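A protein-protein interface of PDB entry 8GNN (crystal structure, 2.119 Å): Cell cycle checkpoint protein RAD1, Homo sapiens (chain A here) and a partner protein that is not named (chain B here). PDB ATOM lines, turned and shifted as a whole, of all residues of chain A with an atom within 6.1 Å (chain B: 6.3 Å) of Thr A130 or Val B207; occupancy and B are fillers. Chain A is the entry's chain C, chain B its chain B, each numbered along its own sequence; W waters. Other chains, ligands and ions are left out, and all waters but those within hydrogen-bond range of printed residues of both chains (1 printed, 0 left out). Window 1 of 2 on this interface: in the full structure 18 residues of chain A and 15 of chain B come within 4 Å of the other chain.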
ATOM      1  N   CYS A  92      -4.843  28.826 -23.738  1.00  0.00           N
ATOM      2  CA  CYS A  92      -6.225  28.371 -23.650  1.00  0.00           C
ATOM      3  C   CYS A  92      -7.006  29.120 -22.575  1.00  0.00           C
ATOM      4  O   CYS A  92      -8.161  29.488 -22.784  1.00  0.00           O
ATOM      5  CB  CYS A  92      -6.274  26.867 -23.373  1.00  0.00           C
ATOM      6  SG  CYS A  92      -5.633  25.840 -24.715  1.00  0.00           S
ATOM      7  N   ILE A  95      -8.080  32.439 -23.860  1.00  0.00           N
ATOM      8  CA  ILE A  95      -8.557  32.307 -25.234  1.00  0.00           C
ATOM      9  C   ILE A  95      -9.530  33.424 -25.624  1.00  0.00           C
ATOM     10  O   ILE A  95      -9.663  33.753 -26.803  1.00  0.00           O
ATOM     11  CB  ILE A  95      -9.238  30.929 -25.456  1.00  0.00           C
ATOM     12  CG1 ILE A  95      -9.457  30.655 -26.947  1.00  0.00           C
ATOM     13  CG2 ILE A  95     -10.540  30.828 -24.673  1.00  0.00           C
ATOM     14  CD1 ILE A  95      -8.178  30.499 -27.737  1.00  0.00           C
ATOM     15  N   PHE A  96     -10.190  34.023 -24.638  1.00  0.00           N
ATOM     16  CA  PHE A  96     -11.167  35.072 -24.917  1.00  0.00           C
ATOM     17  C   PHE A  96     -10.592  36.476 -24.747  1.00  0.00           C
ATOM     18  O   PHE A  96     -11.338  37.450 -24.645  1.00  0.00           O
ATOM     19  CB  PHE A  96     -12.399  34.907 -24.022  1.00  0.00           C
ATOM     20  CG  PHE A  96     -13.294  33.771 -24.425  1.00  0.00           C
ATOM     21  CD1 PHE A  96     -14.021  33.830 -25.603  1.00  0.00           C
ATOM     22  CD2 PHE A  96     -13.418  32.649 -23.623  1.00  0.00           C
ATOM     23  CE1 PHE A  96     -14.848  32.789 -25.978  1.00  0.00           C
ATOM     24  CE2 PHE A  96     -14.246  31.603 -23.992  1.00  0.00           C
ATOM     25  CZ  PHE A  96     -14.962  31.674 -25.171  1.00  0.00           C
ATOM     26  N   LEU A 121     -10.546  21.624 -20.529  1.00  0.00           N
ATOM     27  CA  LEU A 121     -10.859  22.993 -20.145  1.00  0.00           C
ATOM     28  C   LEU A 121     -12.146  23.464 -20.810  1.00  0.00           C
ATOM     29  O   LEU A 121     -12.285  23.399 -22.031  1.00  0.00           O
ATOM     30  CB  LEU A 121      -9.709  23.933 -20.508  1.00  0.00           C
ATOM     31  CG  LEU A 121      -8.328  23.602 -19.939  1.00  0.00           C
ATOM     32  CD1 LEU A 121      -7.316  24.644 -20.383  1.00  0.00           C
ATOM     33  CD2 LEU A 121      -8.377  23.507 -18.424  1.00  0.00           C
ATOM     34  N   PHE A 122     -13.085  23.937 -19.999  1.00  0.00           N
ATOM     35  CA  PHE A 122     -14.333  24.487 -20.509  1.00  0.00           C
ATOM     36  C   PHE A 122     -14.448  25.959 -20.139  1.00  0.00           C
ATOM     37  O   PHE A 122     -14.794  26.300 -19.009  1.00  0.00           O
ATOM     38  CB  PHE A 122     -15.534  23.711 -19.964  1.00  0.00           C
ATOM     39  CG  PHE A 122     -15.581  22.276 -20.403  1.00  0.00           C
ATOM     40  CD1 PHE A 122     -14.896  21.299 -19.700  1.00  0.00           C
ATOM     41  CD2 PHE A 122     -16.312  21.903 -21.519  1.00  0.00           C
ATOM     42  CE1 PHE A 122     -14.938  19.977 -20.100  1.00  0.00           C
ATOM     43  CE2 PHE A 122     -16.358  20.582 -21.925  1.00  0.00           C
ATOM     44  CZ  PHE A 122     -15.671  19.618 -21.215  1.00  0.00           C
ATOM     45  N   LEU A 123     -14.155  26.832 -21.097  1.00  0.00           N
ATOM     46  CA  LEU A 123     -14.217  28.267 -20.853  1.00  0.00           C
ATOM     47  C   LEU A 123     -15.427  28.883 -21.545  1.00  0.00           C
ATOM     48  O   LEU A 123     -15.710  28.586 -22.705  1.00  0.00           O
ATOM     49  CB  LEU A 123     -12.928  28.947 -21.315  1.00  0.00           C
ATOM     50  CG  LEU A 123     -11.649  28.409 -20.664  1.00  0.00           C
ATOM     51  CD1 LEU A 123     -10.934  27.427 -21.584  1.00  0.00           C
ATOM     52  CD2 LEU A 123     -10.724  29.545 -20.254  1.00  0.00           C
ATOM     53  N   GLU A 124     -16.139  29.741 -20.821  1.00  0.00           N
ATOM     54  CA  GLU A 124     -17.363  30.342 -21.334  1.00  0.00           C
ATOM     55  C   GLU A 124     -17.403  31.845 -21.075  1.00  0.00           C
ATOM     56  O   GLU A 124     -17.194  32.298 -19.950  1.00  0.00           O
ATOM     57  CB  GLU A 124     -18.587  29.661 -20.709  1.00  0.00           C
ATOM     58  CG  GLU A 124     -19.932  30.142 -21.242  1.00  0.00           C
ATOM     59  CD  GLU A 124     -20.468  31.350 -20.494  1.00  0.00           C
ATOM     60  OE1 GLU A 124     -20.105  31.528 -19.312  1.00  0.00           O
ATOM     61  OE2 GLU A 124     -21.251  32.120 -21.089  1.00  0.00           O
ATOM     62  N   VAL A 128     -20.664  32.233 -25.441  1.00  0.00           N
ATOM     63  CA  VAL A 128     -19.671  31.592 -26.290  1.00  0.00           C
ATOM     64  C   VAL A 128     -18.851  30.603 -25.471  1.00  0.00           C
ATOM     65  O   VAL A 128     -18.359  30.938 -24.394  1.00  0.00           O
ATOM     66  CB  VAL A 128     -18.734  32.622 -26.946  1.00  0.00           C
ATOM     67  CG1 VAL A 128     -17.810  31.941 -27.941  1.00  0.00           C
ATOM     68  CG2 VAL A 128     -19.543  33.714 -27.629  1.00  0.00           C
ATOM     69  N   VAL A 129     -18.711  29.384 -25.980  1.00  0.00           N
ATOM     70  CA  VAL A 129     -18.020  28.331 -25.248  1.00  0.00           C
ATOM     71  C   VAL A 129     -16.816  27.791 -26.013  1.00  0.00           C
ATOM     72  O   VAL A 129     -16.930  27.395 -27.174  1.00  0.00           O
ATOM     73  CB  VAL A 129     -18.970  27.161 -24.927  1.00  0.00           C
ATOM     74  CG1 VAL A 129     -18.212  26.024 -24.257  1.00  0.00           C
ATOM     75  CG2 VAL A 129     -20.119  27.636 -24.050  1.00  0.00           C
ATOM     76  N   THR A 130     -15.661  27.781 -25.355  1.00  0.00           N
ATOM     77  CA  THR A 130     -14.459  27.190 -25.927  1.00  0.00           C
ATOM     78  C   THR A 130     -14.078  25.926 -25.166  1.00  0.00           C
ATOM     79  O   THR A 130     -13.931  25.947 -23.944  1.00  0.00           O
ATOM     80  CB  THR A 130     -13.274  28.172 -25.911  1.00  0.00           C
ATOM     81  OG1 THR A 130     -13.581  29.310 -26.726  1.00  0.00           O
ATOM     82  CG2 THR A 130     -12.018  27.499 -26.445  1.00  0.00           C
ATOM     83  N   VAL A 131     -13.928  24.825 -25.894  1.00  0.00           N
ATOM     84  CA  VAL A 131     -13.551  23.555 -25.288  1.00  0.00           C
ATOM     85  C   VAL A 131     -12.118  23.189 -25.654  1.00  0.00           C
ATOM     86  O   VAL A 131     -11.777  23.067 -26.832  1.00  0.00           O
ATOM     87  CB  VAL A 131     -14.495  22.419 -25.721  1.00  0.00           C
ATOM     88  CG1 VAL A 131     -14.030  21.092 -25.140  1.00  0.00           C
ATOM     89  CG2 VAL A 131     -15.921  22.726 -25.293  1.00  0.00           C
ATOM     90  N   CYS A 132     -11.281  23.020 -24.637  1.00  0.00           N
ATOM     91  CA  CYS A 132      -9.883  22.675 -24.850  1.00  0.00           C
ATOM     92  C   CYS A 132      -9.573  21.282 -24.318  1.00  0.00           C
ATOM     93  O   CYS A 132     -10.133  20.848 -23.311  1.00  0.00           O
ATOM     94  CB  CYS A 132      -8.968  23.702 -24.183  1.00  0.00           C
ATOM     95  SG  CYS A 132      -9.373  25.419 -24.566  1.00  0.00           S
ATOM     96  N   LYS A 133      -8.676  20.585 -25.003  1.00  0.00           N
ATOM     97  CA  LYS A 133      -8.245  19.268 -24.568  1.00  0.00           C
ATOM     98  C   LYS A 133      -6.732  19.182 -24.762  1.00  0.00           C
ATOM     99  O   LYS A 133      -6.232  19.117 -25.887  1.00  0.00           O
ATOM    100  CB  LYS A 133      -9.008  18.173 -25.331  1.00  0.00           C
ATOM    101  CG  LYS A 133      -8.229  16.915 -25.686  1.00  0.00           C
ATOM    102  CD  LYS A 133      -9.086  15.979 -26.528  1.00  0.00           C
ATOM    103  CE  LYS A 133      -8.236  14.968 -27.273  1.00  0.00           C
ATOM    104  NZ  LYS A 133      -7.123  15.646 -27.989  1.00  0.00           N
ATOM    105  N   VAL B 175     -10.177  35.225 -29.935  1.00  0.00           N
ATOM    106  CA  VAL B 175     -10.078  33.772 -29.981  1.00  0.00           C
ATOM    107  C   VAL B 175      -9.073  33.321 -31.037  1.00  0.00           C
ATOM    108  O   VAL B 175      -8.220  32.474 -30.774  1.00  0.00           O
ATOM    109  CB  VAL B 175     -11.448  33.125 -30.270  1.00  0.00           C
ATOM    110  CG1 VAL B 175     -11.299  31.626 -30.469  1.00  0.00           C
ATOM    111  CG2 VAL B 175     -12.424  33.421 -29.141  1.00  0.00           C
ATOM    112  N   MET B 179      -5.485  31.395 -30.797  1.00  0.00           N
ATOM    113  CA  MET B 179      -5.393  30.118 -31.495  1.00  0.00           C
ATOM    114  C   MET B 179      -4.184  30.106 -32.424  1.00  0.00           C
ATOM    115  O   MET B 179      -3.606  29.052 -32.691  1.00  0.00           O
ATOM    116  CB  MET B 179      -6.673  29.834 -32.286  1.00  0.00           C
ATOM    117  CG  MET B 179      -7.835  29.341 -31.436  1.00  0.00           C
ATOM    118  SD  MET B 179      -9.204  28.684 -32.414  1.00  0.00           S
ATOM    119  CE  MET B 179      -9.678  30.126 -33.363  1.00  0.00           C
ATOM    120  N   ILE B 182      -1.073  28.648 -31.131  1.00  0.00           N
ATOM    121  CA  ILE B 182      -1.059  27.195 -31.028  1.00  0.00           C
ATOM    122  C   ILE B 182      -0.837  26.527 -32.381  1.00  0.00           C
ATOM    123  O   ILE B 182       0.038  25.673 -32.525  1.00  0.00           O
ATOM    124  CB  ILE B 182      -2.370  26.674 -30.418  1.00  0.00           C
ATOM    125  CG1 ILE B 182      -2.526  27.189 -28.984  1.00  0.00           C
ATOM    126  CG2 ILE B 182      -2.409  25.156 -30.451  1.00  0.00           C
ATOM    127  CD1 ILE B 182      -3.814  26.762 -28.317  1.00  0.00           C
ATOM    128  N   LEU B 198     -14.983  27.472 -34.480  1.00  0.00           N
ATOM    129  CA  LEU B 198     -13.596  27.683 -34.875  1.00  0.00           C
ATOM    130  C   LEU B 198     -12.744  26.566 -34.285  1.00  0.00           C
ATOM    131  O   LEU B 198     -12.677  26.411 -33.066  1.00  0.00           O
ATOM    132  CB  LEU B 198     -13.092  29.049 -34.409  1.00  0.00           C
ATOM    133  CG  LEU B 198     -13.830  30.284 -34.932  1.00  0.00           C
ATOM    134  CD1 LEU B 198     -13.258  31.550 -34.311  1.00  0.00           C
ATOM    135  CD2 LEU B 198     -13.762  30.350 -36.451  1.00  0.00           C
ATOM    136  N   LYS B 199     -12.101  25.784 -35.146  1.00  0.00           N
ATOM    137  CA  LYS B 199     -11.366  24.611 -34.685  1.00  0.00           C
ATOM    138  C   LYS B 199      -9.903  24.600 -35.115  1.00  0.00           C
ATOM    139  O   LYS B 199      -9.587  24.748 -36.296  1.00  0.00           O
ATOM    140  CB  LYS B 199     -12.042  23.333 -35.185  1.00  0.00           C
ATOM    141  CG  LYS B 199     -13.437  23.101 -34.634  1.00  0.00           C
ATOM    142  CD  LYS B 199     -13.950  21.717 -34.998  1.00  0.00           C
ATOM    143  CE  LYS B 199     -14.141  21.574 -36.499  1.00  0.00           C
ATOM    144  NZ  LYS B 199     -14.667  20.230 -36.867  1.00  0.00           N
ATOM    145  N   ILE B 200      -9.016  24.427 -34.141  1.00  0.00           N
ATOM    146  CA  ILE B 200      -7.624  24.103 -34.416  1.00  0.00           C
ATOM    147  C   ILE B 200      -7.316  22.766 -33.757  1.00  0.00           C
ATOM    148  O   ILE B 200      -7.912  22.413 -32.738  1.00  0.00           O
ATOM    149  CB  ILE B 200      -6.651  25.186 -33.908  1.00  0.00           C
ATOM    150  CG1 ILE B 200      -6.728  25.314 -32.387  1.00  0.00           C
ATOM    151  CG2 ILE B 200      -6.939  26.521 -34.576  1.00  0.00           C
ATOM    152  CD1 ILE B 200      -5.744  26.304 -31.811  1.00  0.00           C
ATOM    153  N   GLU B 201      -6.395  22.012 -34.346  1.00  0.00           N
ATOM    154  CA  GLU B 201      -6.117  20.667 -33.866  1.00  0.00           C
ATOM    155  C   GLU B 201      -4.684  20.252 -34.156  1.00  0.00           C
ATOM    156  O   GLU B 201      -4.271  20.156 -35.313  1.00  0.00           O
ATOM    157  CB  GLU B 201      -7.097  19.673 -34.492  1.00  0.00           C
ATOM    158  CG  GLU B 201      -6.879  18.227 -34.083  1.00  0.00           C
ATOM    159  CD  GLU B 201      -8.074  17.349 -34.402  1.00  0.00           C
ATOM    160  OE1 GLU B 201      -9.020  17.845 -35.050  1.00  0.00           O
ATOM    161  OE2 GLU B 201      -8.069  16.165 -34.005  1.00  0.00           O
ATOM    162  N   THR B 202      -3.926  20.017 -33.090  1.00  0.00           N
ATOM    163  CA  THR B 202      -2.554  19.549 -33.205  1.00  0.00           C
ATOM    164  C   THR B 202      -2.409  18.219 -32.471  1.00  0.00           C
ATOM    165  O   THR B 202      -3.383  17.688 -31.939  1.00  0.00           O
ATOM    166  CB  THR B 202      -1.552  20.570 -32.634  1.00  0.00           C
ATOM    167  OG1 THR B 202      -1.632  20.574 -31.203  1.00  0.00           O
ATOM    168  CG2 THR B 202      -1.850  21.967 -33.163  1.00  0.00           C
ATOM    169  N   VAL B 205      -2.799  19.345 -28.605  1.00  0.00           N
ATOM    170  CA  VAL B 205      -3.981  20.046 -28.112  1.00  0.00           C
ATOM    171  C   VAL B 205      -5.045  20.291 -29.186  1.00  0.00           C
ATOM    172  O   VAL B 205      -4.732  20.657 -30.319  1.00  0.00           O
ATOM    173  CB  VAL B 205      -3.577  21.402 -27.480  1.00  0.00           C
ATOM    174  CG1 VAL B 205      -2.640  22.166 -28.405  1.00  0.00           C
ATOM    175  CG2 VAL B 205      -4.802  22.237 -27.127  1.00  0.00           C
ATOM    176  N   CYS B 206      -6.305  20.074 -28.817  1.00  0.00           N
ATOM    177  CA  CYS B 206      -7.436  20.435 -29.665  1.00  0.00           C
ATOM    178  C   CYS B 206      -8.220  21.579 -29.030  1.00  0.00           C
ATOM    179  O   CYS B 206      -8.534  21.538 -27.842  1.00  0.00           O
ATOM    180  CB  CYS B 206      -8.353  19.232 -29.892  1.00  0.00           C
ATOM    181  SG  CYS B 206      -7.541  17.789 -30.610  1.00  0.00           S
ATOM    182  N   VAL B 207      -8.529  22.602 -29.821  1.00  0.00           N
ATOM    183  CA  VAL B 207      -9.308  23.733 -29.327  1.00  0.00           C
ATOM    184  C   VAL B 207     -10.496  24.021 -30.236  1.00  0.00           C
ATOM    185  O   VAL B 207     -10.336  24.212 -31.442  1.00  0.00           O
ATOM    186  CB  VAL B 207      -8.451  25.009 -29.202  1.00  0.00           C
ATOM    187  CG1 VAL B 207      -9.301  26.171 -28.711  1.00  0.00           C
ATOM    188  CG2 VAL B 207      -7.276  24.776 -28.267  1.00  0.00           C
ATOM    189  N   THR B 208     -11.688  24.048 -29.651  1.00  0.00           N
ATOM    190  CA  THR B 208     -12.905  24.342 -30.398  1.00  0.00           C
ATOM    191  C   THR B 208     -13.729  25.419 -29.702  1.00  0.00           C
ATOM    192  O   THR B 208     -14.103  25.270 -28.540  1.00  0.00           O
ATOM    193  CB  THR B 208     -13.774  23.083 -30.580  1.00  0.00           C
ATOM    194  OG1 THR B 208     -13.018  22.069 -31.253  1.00  0.00           O
ATOM    195  CG2 THR B 208     -15.019  23.409 -31.390  1.00  0.00           C
ATOM    196  N   THR B 209     -14.006  26.502 -30.418  1.00  0.00           N
ATOM    197  CA  THR B 209     -14.828  27.581 -29.884  1.00  0.00           C
ATOM    198  C   THR B 209     -16.219  27.544 -30.509  1.00  0.00           C
ATOM    199  O   THR B 209     -16.361  27.578 -31.731  1.00  0.00           O
ATOM    200  CB  THR B 209     -14.185  28.955 -30.133  1.00  0.00           C
ATOM    201  OG1 THR B 209     -12.918  29.015 -29.466  1.00  0.00           O
ATOM    202  CG2 THR B 209     -15.078  30.064 -29.603  1.00  0.00           C
ATOM    203  N   HIS B 210     -17.243  27.476 -29.664  1.00  0.00           N
ATOM    204  CA  HIS B 210     -18.615  27.318 -30.133  1.00  0.00           C
ATOM    205  C   HIS B 210     -19.425  28.609 -30.068  1.00  0.00           C
ATOM    206  O   HIS B 210     -19.681  29.141 -28.987  1.00  0.00           O
ATOM    207  CB  HIS B 210     -19.330  26.234 -29.323  1.00  0.00           C
ATOM    208  CG  HIS B 210     -18.734  24.869 -29.478  1.00  0.00           C
ATOM    209  ND1 HIS B 210     -19.020  24.052 -30.550  1.00  0.00           N
ATOM    210  CD2 HIS B 210     -17.873  24.177 -28.695  1.00  0.00           C
ATOM    211  CE1 HIS B 210     -18.358  22.915 -30.422  1.00  0.00           C
ATOM    212  NE2 HIS B 210     -17.656  22.966 -29.305  1.00  0.00           N
HETATM  213  O   HOH W   1     -21.679  28.243 -27.096  1.00  0.00           O
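The backbone carbonyl oxygen of Leu B198 is in hydrogen-bond range of the backbone NH of Thr B209 (3.0 Å). The backbone carbonyl oxygen of Ile B200 lies within hydrogen-bond range of the backbone NH of Val B207 (3.0 Å). OG1 of Thr B202 lies within hydrogen-bond range of N of Val B205 (3.1 Å). The side-chain sulfur (SG) of Cys A92 sits close to the side-chain sulfur (SG) of Cys A132, 3.8 Å away. N of Cys A132 sits at hydrogen-bond distance from O of Leu A121 (2.8 Å). N of Thr A130 is in hydrogen-bond range of O of Leu A123, at 2.8 Å.
Water W1 bridges the backbone carbonyl oxygen of His B210 and the backbone NH of Val A129.
Of the 13 printed residues of chain A, 8 touch a printed residue of chain B. Printed residues of chain A that touch a printed residue of chain B: Ile A95, Phe A96, Val A128, Val A129, Thr A130, Val A131, Cys A132 and Lys A133. Hydrophobic or aromatic side chains of chain A within 4 Å of the printed part of chain B: Ile A95, Phe A96 and Val A128. Of the 14 printed residues of chain B, 8 touch a printed residue of chain A. Printed residues of chain B that touch a printed residue of chain A: Val B175, Met B179, Val B205, Cys B206, Val B207, Thr B208, Thr B209 and His B210. Hydrophobic or aromatic side chains of chain B that line the printed part of chain A: Val B175, Met B179, Val B205, Val B207 and His B210.
The backbone carbonyl oxygen (O) of Ile A95 lies close to the backbone NH (N) of Val B175. O of Cys B206 lies within hydrogen-bond range of N of Lys A133 (3.0 Å). The backbone NH (N) of Val A131 is in hydrogen-bond range of the backbone carbonyl oxygen (O) of Thr B208 (2.7 Å). The side-chain hydroxyl (OG1) of Thr B209 lies within hydrogen-bond range of the side-chain hydroxyl (OG1) of Thr A130. The backbone NH (N) of His B210 is in hydrogen-bond range of the backbone carbonyl oxygen (O) of Val A129, at 2.5 Å.
Phe A96 touches Val B175. Val A128 touches Thr B209 (CG1 to CG2, 3.7 Å). Val A128 touches His B210. Val A129 touches Thr B208 (O to O, 3.8 Å). Val A129 touches Thr B209. CG2 of Thr A130 touches CG1 of Val B207, 3.8 Å away. Thr A130 touches Thr B208 (CA to O, 3.3 Å). Cys B206 touches Val A131 (O to O, 3.7 Å). Val B207 touches Val A131 (CA to O, 3.6 Å). Lys A133 touches Val B205.
Of chain B, only Val B207 (3.8 Å), Thr B208 (3.3 Å) and Thr B209 (2.8 Å) come within 4 Å of Thr A130. Of chain A, only Thr A130 and Val A131 come within 4 Å of Val B207. Of the printed residues of chain A, Thr B208 touches Val A129, Thr A130 and Val A131. Printed residues of chain B within 4 Å of Lys A133: Val B205 (3.3 Å) and Cys B206 (3.0 Å). Cys A92 touches none of the printed residues of chain B. The nearest residue of chain B that does not touch Thr A130 is His B210 (4.6 Å).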
